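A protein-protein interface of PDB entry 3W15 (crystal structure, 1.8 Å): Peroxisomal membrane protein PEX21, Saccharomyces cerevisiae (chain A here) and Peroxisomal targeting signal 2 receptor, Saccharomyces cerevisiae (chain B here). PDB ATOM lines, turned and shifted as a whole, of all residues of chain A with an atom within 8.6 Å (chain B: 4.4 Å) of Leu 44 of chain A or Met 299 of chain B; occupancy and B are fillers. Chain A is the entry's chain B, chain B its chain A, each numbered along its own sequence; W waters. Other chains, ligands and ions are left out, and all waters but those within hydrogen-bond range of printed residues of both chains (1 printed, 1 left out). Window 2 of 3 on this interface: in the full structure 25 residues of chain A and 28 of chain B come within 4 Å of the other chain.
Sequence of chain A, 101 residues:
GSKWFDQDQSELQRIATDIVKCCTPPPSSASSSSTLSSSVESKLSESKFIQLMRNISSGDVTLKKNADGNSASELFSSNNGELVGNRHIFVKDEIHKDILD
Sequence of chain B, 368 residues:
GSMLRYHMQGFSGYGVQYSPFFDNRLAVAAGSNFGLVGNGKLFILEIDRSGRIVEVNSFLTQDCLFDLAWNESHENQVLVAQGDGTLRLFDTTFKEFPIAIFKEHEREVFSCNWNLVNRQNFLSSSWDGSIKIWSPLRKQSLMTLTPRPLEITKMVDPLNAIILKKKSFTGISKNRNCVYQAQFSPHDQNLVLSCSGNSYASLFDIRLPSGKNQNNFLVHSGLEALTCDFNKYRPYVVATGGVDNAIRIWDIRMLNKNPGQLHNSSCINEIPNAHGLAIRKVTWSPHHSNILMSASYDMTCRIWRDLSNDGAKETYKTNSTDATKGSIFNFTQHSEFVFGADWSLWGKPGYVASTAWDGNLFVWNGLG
The backbone NH (N) of Phe 49 of chain A lies within hydrogen-bond range of the side-chain carboxylate (OE1) of Glu 336 of chain B (3.4 Å). The backbone carbonyl oxygen (O) of His 334 of chain B lies within hydrogen-bond range of the side-chain amino group (NZ) of Lys 43 of chain A, at 2.9 Å. OE1 of Glu 336 of chain B sits at hydrogen-bond distance from OG of Ser 47 of chain A. The side-chain carboxylate (OE2) of Glu 336 of chain B lies within hydrogen-bond range of the backbone NH (N) of Lys 48 of chain A (2.6 Å). O of Met 299 of chain B sits at hydrogen-bond distance from NZ of Lys 43 of chain A, 3.3 Å away.
The backbone NH of Ile 50 of chain A lies within hydrogen-bond range of the side-chain hydroxyl of Ser 47 of chain A (3.1 Å). SG of Cys 22 of chain A is disulfide-bonded to SG of Cys 23 of chain A (2.0 Å). The side-chain sulfur (SD) of Met 299 of chain B sits close to the backbone NH (N) of Glu 336 of chain B, at 3.7 Å. OG of Ser 47 of chain A is in hydrogen-bond range of N of Phe 49 of chain A (3.1 Å).
Among the printed residues, merely in contact across the chains: Leu 44 of chain A with Met 299 of chain B (3.9 Å) and Phe 49 of chain A with Phe 337 of chain B (3.6 Å).
Of chain B, only Met 299 (3.9 Å) comes within 4 Å of Leu 44 of chain A. Printed residues of chain A within 4 Å of Met 299 of chain B: Lys 43 and Leu 44. Of the printed residues of chain B, Phe 49 of chain A touches Glu 336 and Phe 337. Printed residues of chain B within 4 Å of Lys 48 of chain A: Glu 336. The nearest residue of chain B that does not touch Leu 44 of chain A is Phe 337 of chain B (4.3 Å). The nearest residue of chain A that does not touch Met 299 of chain B is Ser 47 of chain A (4.2 Å).
Of the 11 printed residues of chain B, 4 touch a printed residue of chain A. Hydrophobic or aromatic side chains of chain A that line the printed part of chain B: Leu 44 and Phe 49. Among the printed residues, 7 pairs touch across the chains.
Water W1 bridges NZ of Lys 43 of chain A (2.8 Å) and O of Asp 298 of chain B (3.0 Å).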
ATOM      1  N   ILE A  19       6.412  -3.513  12.665  1.00  0.00           N
ATOM      2  CA  ILE A  19       5.623  -2.411  13.227  1.00  0.00           C
ATOM      3  C   ILE A  19       6.536  -1.364  13.876  1.00  0.00           C
ATOM      4  O   ILE A  19       6.341  -0.157  13.691  1.00  0.00           O
ATOM      5  CB  ILE A  19       4.561  -2.917  14.249  1.00  0.00           C
ATOM      6  CG1 ILE A  19       3.483  -3.731  13.529  1.00  0.00           C
ATOM      7  CG2 ILE A  19       3.938  -1.744  15.018  1.00  0.00           C
ATOM      8  CD1 ILE A  19       2.504  -4.460  14.438  1.00  0.00           C
ATOM      9  N   CYS A  22       8.287   0.497  10.898  1.00  0.00           N
ATOM     10  CA  CYS A  22       7.420   1.385  10.112  1.00  0.00           C
ATOM     11  C   CYS A  22       7.056   2.666  10.845  1.00  0.00           C
ATOM     12  O   CYS A  22       7.088   3.753  10.266  1.00  0.00           O
ATOM     13  CB  CYS A  22       6.128   0.676   9.662  1.00  0.00           C
ATOM     14  SG  CYS A  22       4.785   0.494  10.916  1.00  0.00           S
ATOM     15  N   CYS A  23       6.718   2.530  12.123  1.00  0.00           N
ATOM     16  CA  CYS A  23       5.847   3.502  12.765  1.00  0.00           C
ATOM     17  C   CYS A  23       6.267   3.891  14.192  1.00  0.00           C
ATOM     18  O   CYS A  23       5.461   3.829  15.126  1.00  0.00           O
ATOM     19  CB  CYS A  23       4.409   2.960  12.726  1.00  0.00           C
ATOM     20  SG  CYS A  23       3.901   2.330  11.074  1.00  0.00           S
ATOM     21  N   THR A  24       7.528   4.295  14.351  1.00  0.00           N
ATOM     22  CA  THR A  24       8.035   4.808  15.630  1.00  0.00           C
ATOM     23  C   THR A  24       8.903   6.047  15.419  1.00  0.00           C
ATOM     24  O   THR A  24       9.547   6.540  16.349  1.00  0.00           O
ATOM     25  CB  THR A  24       8.854   3.748  16.420  1.00  0.00           C
ATOM     26  OG1 THR A  24       9.890   3.215  15.585  1.00  0.00           O
ATOM     27  CG2 THR A  24       7.968   2.620  16.915  1.00  0.00           C
ATOM     28  N   SER A  37       2.250  14.219  11.206  1.00  0.00           N
ATOM     29  CA  SER A  37       1.908  15.249  12.181  1.00  0.00           C
ATOM     30  C   SER A  37       2.666  15.070  13.500  1.00  0.00           C
ATOM     31  O   SER A  37       2.831  13.947  13.984  1.00  0.00           O
ATOM     32  CB  SER A  37       0.397  15.265  12.432  1.00  0.00           C
ATOM     33  OG  SER A  37       0.067  16.091  13.538  1.00  0.00           O
ATOM     34  N   SER A  38       3.115  16.188  14.069  1.00  0.00           N
ATOM     35  CA  SER A  38       3.876  16.203  15.326  1.00  0.00           C
ATOM     36  C   SER A  38       3.132  15.532  16.487  1.00  0.00           C
ATOM     37  O   SER A  38       3.710  14.730  17.228  1.00  0.00           O
ATOM     38  CB  SER A  38       4.259  17.643  15.697  1.00  0.00           C
ATOM     39  OG  SER A  38       4.674  17.738  17.050  1.00  0.00           O
ATOM     40  N   SER A  39       1.853  15.871  16.634  1.00  0.00           N
ATOM     41  CA  SER A  39       1.004  15.311  17.684  1.00  0.00           C
ATOM     42  C   SER A  39       0.900  13.789  17.580  1.00  0.00           C
ATOM     43  O   SER A  39       1.004  13.082  18.587  1.00  0.00           O
ATOM     44  CB  SER A  39      -0.390  15.936  17.628  1.00  0.00           C
ATOM     45  OG  SER A  39      -0.329  17.340  17.786  1.00  0.00           O
ATOM     46  N   VAL A  40       0.707  13.300  16.355  1.00  0.00           N
ATOM     47  CA  VAL A  40       0.556  11.869  16.088  1.00  0.00           C
ATOM     48  C   VAL A  40       1.850  11.108  16.380  1.00  0.00           C
ATOM     49  O   VAL A  40       1.827  10.052  17.020  1.00  0.00           O
ATOM     50  CB  VAL A  40       0.103  11.603  14.622  1.00  0.00           C
ATOM     51  CG1 VAL A  40      -0.193  10.124  14.404  1.00  0.00           C
ATOM     52  CG2 VAL A  40      -1.122  12.443  14.275  1.00  0.00           C
ATOM     53  N   GLU A  41       2.972  11.652  15.909  1.00  0.00           N
ATOM     54  CA  GLU A  41       4.283  11.030  16.103  1.00  0.00           C
ATOM     55  C   GLU A  41       4.609  10.859  17.584  1.00  0.00           C
ATOM     56  O   GLU A  41       5.081   9.800  18.001  1.00  0.00           O
ATOM     57  CB  GLU A  41       5.382  11.836  15.399  1.00  0.00           C
ATOM     58  N   SER A  42       4.338  11.897  18.375  1.00  0.00           N
ATOM     59  CA  SER A  42       4.577  11.844  19.813  1.00  0.00           C
ATOM     60  C   SER A  42       3.662  10.820  20.488  1.00  0.00           C
ATOM     61  O   SER A  42       4.094  10.097  21.386  1.00  0.00           O
ATOM     62  CB  SER A  42       4.428  13.231  20.452  1.00  0.00           C
ATOM     63  OG  SER A  42       3.086  13.679  20.419  1.00  0.00           O
ATOM     64  N   LYS A  43       2.408  10.758  20.036  1.00  0.00           N
ATOM     65  CA  LYS A  43       1.436   9.789  20.546  1.00  0.00           C
ATOM     66  C   LYS A  43       1.872   8.346  20.289  1.00  0.00           C
ATOM     67  O   LYS A  43       1.734   7.486  21.163  1.00  0.00           O
ATOM     68  CB  LYS A  43       0.053  10.033  19.942  1.00  0.00           C
ATOM     69  CG  LYS A  43      -0.770  11.103  20.641  1.00  0.00           C
ATOM     70  CD  LYS A  43      -2.241  10.884  20.334  1.00  0.00           C
ATOM     71  CE  LYS A  43      -3.115  12.025  20.815  1.00  0.00           C
ATOM     72  NZ  LYS A  43      -4.481  11.904  20.219  1.00  0.00           N
ATOM     73  N   LEU A  44       2.402   8.093  19.093  1.00  0.00           N
ATOM     74  CA  LEU A  44       2.965   6.787  18.752  1.00  0.00           C
ATOM     75  C   LEU A  44       4.191   6.442  19.594  1.00  0.00           C
ATOM     76  O   LEU A  44       4.350   5.298  20.025  1.00  0.00           O
ATOM     77  CB  LEU A  44       3.318   6.714  17.263  1.00  0.00           C
ATOM     78  CG  LEU A  44       2.211   6.377  16.264  1.00  0.00           C
ATOM     79  CD1 LEU A  44       2.732   6.567  14.853  1.00  0.00           C
ATOM     80  CD2 LEU A  44       1.698   4.956  16.462  1.00  0.00           C
ATOM     81  N   SER A  45       5.055   7.432  19.828  1.00  0.00           N
ATOM     82  CA  SER A  45       6.266   7.211  20.622  1.00  0.00           C
ATOM     83  C   SER A  45       5.935   6.860  22.071  1.00  0.00           C
ATOM     84  O   SER A  45       6.641   6.072  22.700  1.00  0.00           O
ATOM     85  CB  SER A  45       7.209   8.420  20.553  1.00  0.00           C
ATOM     86  OG  SER A  45       6.691   9.535  21.261  1.00  0.00           O
ATOM     87  N   GLU A  46       4.848   7.433  22.585  1.00  0.00           N
ATOM     88  CA  GLU A  46       4.418   7.186  23.960  1.00  0.00           C
ATOM     89  C   GLU A  46       3.365   6.078  24.091  1.00  0.00           C
ATOM     90  O   GLU A  46       2.847   5.840  25.184  1.00  0.00           O
ATOM     91  CB  GLU A  46       3.913   8.483  24.604  1.00  0.00           C
ATOM     92  CG  GLU A  46       5.020   9.348  25.207  1.00  0.00           C
ATOM     93  CD  GLU A  46       5.583   8.775  26.498  1.00  0.00           C
ATOM     94  OE1 GLU A  46       4.891   8.848  27.540  1.00  0.00           O
ATOM     95  OE2 GLU A  46       6.723   8.258  26.472  1.00  0.00           O
ATOM     96  N   SER A  47       3.071   5.394  22.986  1.00  0.00           N
ATOM     97  CA  SER A  47       1.995   4.395  22.946  1.00  0.00           C
ATOM     98  C   SER A  47       2.323   3.103  23.695  1.00  0.00           C
ATOM     99  O   SER A  47       3.444   2.596  23.618  1.00  0.00           O
ATOM    100  CB  SER A  47       1.619   4.089  21.491  1.00  0.00           C
ATOM    101  OG  SER A  47       1.016   2.817  21.362  1.00  0.00           O
ATOM    102  N   LYS A  48       1.328   2.578  24.410  1.00  0.00           N
ATOM    103  CA  LYS A  48       1.439   1.295  25.112  1.00  0.00           C
ATOM    104  C   LYS A  48       1.420   0.098  24.165  1.00  0.00           C
ATOM    105  O   LYS A  48       2.002  -0.945  24.463  1.00  0.00           O
ATOM    106  CB  LYS A  48       0.333   1.149  26.161  1.00  0.00           C
ATOM    107  CG  LYS A  48       0.518   2.046  27.384  1.00  0.00           C
ATOM    108  CD  LYS A  48       1.602   1.487  28.305  1.00  0.00           C
ATOM    109  CE  LYS A  48       2.436   2.596  28.937  1.00  0.00           C
ATOM    110  NZ  LYS A  48       1.609   3.570  29.705  1.00  0.00           N
ATOM    111  N   PHE A  49       0.740   0.244  23.030  1.00  0.00           N
ATOM    112  CA  PHE A  49       0.778  -0.777  21.996  1.00  0.00           C
ATOM    113  C   PHE A  49       2.192  -0.887  21.417  1.00  0.00           C
ATOM    114  O   PHE A  49       2.743  -1.987  21.276  1.00  0.00           O
ATOM    115  CB  PHE A  49      -0.241  -0.476  20.889  1.00  0.00           C
ATOM    116  CG  PHE A  49      -0.096  -1.359  19.681  1.00  0.00           C
ATOM    117  CD1 PHE A  49      -0.348  -2.726  19.766  1.00  0.00           C
ATOM    118  CD2 PHE A  49       0.301  -0.822  18.457  1.00  0.00           C
ATOM    119  CE1 PHE A  49      -0.204  -3.553  18.647  1.00  0.00           C
ATOM    120  CE2 PHE A  49       0.450  -1.640  17.333  1.00  0.00           C
ATOM    121  CZ  PHE A  49       0.200  -3.004  17.430  1.00  0.00           C
ATOM    122  N   ILE A  50       2.771   0.268  21.100  1.00  0.00           N
ATOM    123  CA  ILE A  50       4.125   0.345  20.548  1.00  0.00           C
ATOM    124  C   ILE A  50       5.166  -0.205  21.536  1.00  0.00           C
ATOM    125  O   ILE A  50       6.101  -0.893  21.130  1.00  0.00           O
ATOM    126  CB  ILE A  50       4.466   1.788  20.092  1.00  0.00           C
ATOM    127  CG1 ILE A  50       3.574   2.211  18.910  1.00  0.00           C
ATOM    128  CG2 ILE A  50       5.960   1.936  19.745  1.00  0.00           C
ATOM    129  CD1 ILE A  50       3.672   1.317  17.654  1.00  0.00           C
ATOM    130  N   GLN A  51       4.978   0.083  22.823  1.00  0.00           N
ATOM    131  CA  GLN A  51       5.819  -0.478  23.885  1.00  0.00           C
ATOM    132  C   GLN A  51       5.758  -2.003  23.913  1.00  0.00           C
ATOM    133  O   GLN A  51       6.783  -2.667  24.100  1.00  0.00           O
ATOM    134  CB  GLN A  51       5.425   0.101  25.247  1.00  0.00           C
ATOM    135  CG  GLN A  51       6.022  -0.641  26.451  1.00  0.00           C
ATOM    136  CD  GLN A  51       5.624  -0.028  27.782  1.00  0.00           C
ATOM    137  OE1 GLN A  51       6.175   0.991  28.199  1.00  0.00           O
ATOM    138  NE2 GLN A  51       4.671  -0.658  28.465  1.00  0.00           N
ATOM    139  N   ARG A  54       7.736  -3.340  20.953  1.00  0.00           N
ATOM    140  CA  ARG A  54       9.170  -3.330  21.270  1.00  0.00           C
ATOM    141  C   ARG A  54       9.556  -4.558  22.094  1.00  0.00           C
ATOM    142  O   ARG A  54      10.521  -5.251  21.769  1.00  0.00           O
ATOM    143  CB  ARG A  54       9.563  -2.058  22.029  1.00  0.00           C
ATOM    144  CG  ARG A  54       9.494  -0.776  21.212  1.00  0.00           C
ATOM    145  CD  ARG A  54      10.056   0.397  22.007  1.00  0.00           C
ATOM    146  NE  ARG A  54       9.680   1.696  21.444  1.00  0.00           N
ATOM    147  CZ  ARG A  54       8.802   2.537  21.993  1.00  0.00           C
ATOM    148  NH1 ARG A  54       8.193   2.235  23.135  1.00  0.00           N
ATOM    149  NH2 ARG A  54       8.532   3.693  21.397  1.00  0.00           N
ATOM    150  N   LEU B 277      -3.300   8.131   9.363  1.00  0.00           N
ATOM    151  CA  LEU B 277      -3.168   6.681   9.313  1.00  0.00           C
ATOM    152  C   LEU B 277      -4.557   6.084   9.046  1.00  0.00           C
ATOM    153  O   LEU B 277      -5.526   6.828   8.963  1.00  0.00           O
ATOM    154  CB  LEU B 277      -2.567   6.139  10.616  1.00  0.00           C
ATOM    155  CG  LEU B 277      -1.084   6.421  10.927  1.00  0.00           C
ATOM    156  CD1 LEU B 277      -0.714   5.835  12.280  1.00  0.00           C
ATOM    157  CD2 LEU B 277      -0.151   5.880   9.838  1.00  0.00           C
ATOM    158  N   SER B 296      -9.783   6.726  13.705  1.00  0.00           N
ATOM    159  CA  SER B 296      -8.561   6.332  12.995  1.00  0.00           C
ATOM    160  C   SER B 296      -7.431   5.808  13.880  1.00  0.00           C
ATOM    161  O   SER B 296      -7.356   6.110  15.079  1.00  0.00           O
ATOM    162  CB  SER B 296      -8.061   7.522  12.157  1.00  0.00           C
ATOM    163  OG  SER B 296      -6.769   7.315  11.603  1.00  0.00           O
ATOM    164  N   TYR B 297      -6.550   5.030  13.255  1.00  0.00           N
ATOM    165  CA  TYR B 297      -5.281   4.602  13.851  1.00  0.00           C
ATOM    166  C   TYR B 297      -4.378   5.804  14.178  1.00  0.00           C
ATOM    167  O   TYR B 297      -3.422   5.665  14.941  1.00  0.00           O
ATOM    168  CB  TYR B 297      -4.529   3.662  12.901  1.00  0.00           C
ATOM    169  CG  TYR B 297      -5.087   2.256  12.745  1.00  0.00           C
ATOM    170  CD1 TYR B 297      -6.129   1.992  11.851  1.00  0.00           C
ATOM    171  CD2 TYR B 297      -4.536   1.183  13.442  1.00  0.00           C
ATOM    172  CE1 TYR B 297      -6.628   0.696  11.686  1.00  0.00           C
ATOM    173  CE2 TYR B 297      -5.030  -0.114  13.282  1.00  0.00           C
ATOM    174  CZ  TYR B 297      -6.073  -0.346  12.401  1.00  0.00           C
ATOM    175  OH  TYR B 297      -6.569  -1.617  12.239  1.00  0.00           O
ATOM    176  N   ASP B 298      -4.670   6.978  13.618  1.00  0.00           N
ATOM    177  CA  ASP B 298      -3.937   8.188  14.019  1.00  0.00           C
ATOM    178  C   ASP B 298      -4.393   8.724  15.387  1.00  0.00           C
ATOM    179  O   ASP B 298      -3.980   9.814  15.816  1.00  0.00           O
ATOM    180  CB  ASP B 298      -3.928   9.272  12.920  1.00  0.00           C
ATOM    181  CG  ASP B 298      -5.239  10.051  12.816  1.00  0.00           C
ATOM    182  OD1 ASP B 298      -6.175   9.820  13.605  1.00  0.00           O
ATOM    183  OD2 ASP B 298      -5.320  10.924  11.928  1.00  0.00           O
ATOM    184  N   MET B 299      -5.254   7.946  16.056  1.00  0.00           N
ATOM    185  CA  MET B 299      -5.682   8.195  17.441  1.00  0.00           C
ATOM    186  C   MET B 299      -6.561   9.429  17.593  1.00  0.00           C
ATOM    187  O   MET B 299      -6.652  10.010  18.679  1.00  0.00           O
ATOM    188  CB  MET B 299      -4.480   8.262  18.395  1.00  0.00           C
ATOM    189  CG  MET B 299      -3.530   7.101  18.241  1.00  0.00           C
ATOM    190  SD  MET B 299      -2.223   7.107  19.470  1.00  0.00           S
ATOM    191  CE  MET B 299      -1.253   5.715  18.908  1.00  0.00           C
ATOM    192  N   THR B 300      -7.219   9.816  16.506  1.00  0.00           N
ATOM    193  CA  THR B 300      -8.186  10.906  16.545  1.00  0.00           C
ATOM    194  C   THR B 300      -9.556  10.450  16.079  1.00  0.00           C
ATOM    195  O   THR B 300      -9.702   9.404  15.436  1.00  0.00           O
ATOM    196  CB  THR B 300      -7.792  12.106  15.654  1.00  0.00           C
ATOM    197  OG1 THR B 300      -7.897  11.743  14.269  1.00  0.00           O
ATOM    198  CG2 THR B 300      -6.386  12.612  15.965  1.00  0.00           C
ATOM    199  N   HIS B 334      -7.943  10.528  22.974  1.00  0.00           N
ATOM    200  CA  HIS B 334      -7.497   9.134  22.998  1.00  0.00           C
ATOM    201  C   HIS B 334      -5.988   9.032  22.789  1.00  0.00           C
ATOM    202  O   HIS B 334      -5.414   9.773  21.994  1.00  0.00           O
ATOM    203  CB  HIS B 334      -8.238   8.295  21.950  1.00  0.00           C
ATOM    204  CG  HIS B 334      -9.670   8.023  22.292  1.00  0.00           C
ATOM    205  ND1 HIS B 334     -10.044   7.227  23.355  1.00  0.00           N
ATOM    206  CD2 HIS B 334     -10.819   8.429  21.704  1.00  0.00           C
ATOM    207  CE1 HIS B 334     -11.361   7.161  23.411  1.00  0.00           C
ATOM    208  NE2 HIS B 334     -11.858   7.883  22.421  1.00  0.00           N
ATOM    209  N   SER B 335      -5.354   8.116  23.514  1.00  0.00           N
ATOM    210  CA  SER B 335      -3.905   7.951  23.464  1.00  0.00           C
ATOM    211  C   SER B 335      -3.461   6.674  22.753  1.00  0.00           C
ATOM    212  O   SER B 335      -2.266   6.357  22.730  1.00  0.00           O
ATOM    213  CB  SER B 335      -3.325   7.988  24.881  1.00  0.00           C
ATOM    214  OG  SER B 335      -3.782   6.869  25.629  1.00  0.00           O
ATOM    215  N   GLU B 336      -4.421   5.932  22.199  1.00  0.00           N
ATOM    216  CA  GLU B 336      -4.148   4.756  21.361  1.00  0.00           C
ATOM    217  C   GLU B 336      -5.152   4.752  20.201  1.00  0.00           C
ATOM    218  O   GLU B 336      -6.013   5.636  20.119  1.00  0.00           O
ATOM    219  CB  GLU B 336      -4.258   3.438  22.148  1.00  0.00           C
ATOM    220  CG  GLU B 336      -3.448   3.340  23.446  1.00  0.00           C
ATOM    221  CD  GLU B 336      -1.964   3.092  23.222  1.00  0.00           C
ATOM    222  OE1 GLU B 336      -1.580   2.585  22.146  1.00  0.00           O
ATOM    223  OE2 GLU B 336      -1.175   3.401  24.141  1.00  0.00           O
ATOM    224  N   PHE B 337      -5.051   3.760  19.317  1.00  0.00           N
ATOM    225  CA  PHE B 337      -5.889   3.707  18.111  1.00  0.00           C
ATOM    226  C   PHE B 337      -7.373   3.819  18.470  1.00  0.00           C
ATOM    227  O   PHE B 337      -7.824   3.151  19.399  1.00  0.00           O
ATOM    228  CB  PHE B 337      -5.666   2.395  17.351  1.00  0.00           C
ATOM    229  CG  PHE B 337      -4.231   2.126  16.967  1.00  0.00           C
ATOM    230  CD1 PHE B 337      -3.359   3.160  16.652  1.00  0.00           C
ATOM    231  CD2 PHE B 337      -3.771   0.820  16.890  1.00  0.00           C
ATOM    232  CE1 PHE B 337      -2.035   2.891  16.286  1.00  0.00           C
ATOM    233  CE2 PHE B 337      -2.457   0.538  16.520  1.00  0.00           C
ATOM    234  CZ  PHE B 337      -1.589   1.576  16.222  1.00  0.00           C
ATOM    235  N   VAL B 338      -8.127   4.645  17.744  1.00  0.00           N
ATOM    236  CA  VAL B 338      -9.580   4.734  17.971  1.00  0.00           C
ATOM    237  C   VAL B 338     -10.353   3.794  17.033  1.00  0.00           C
ATOM    238  O   VAL B 338     -10.331   3.958  15.804  1.00  0.00           O
ATOM    239  CB  VAL B 338     -10.118   6.181  17.872  1.00  0.00           C
ATOM    240  CG1 VAL B 338     -11.555   6.256  18.417  1.00  0.00           C
ATOM    241  CG2 VAL B 338      -9.216   7.156  18.633  1.00  0.00           C
HETATM  242  O   HOH W   1      -3.415  12.100  17.623  1.00  0.00           O
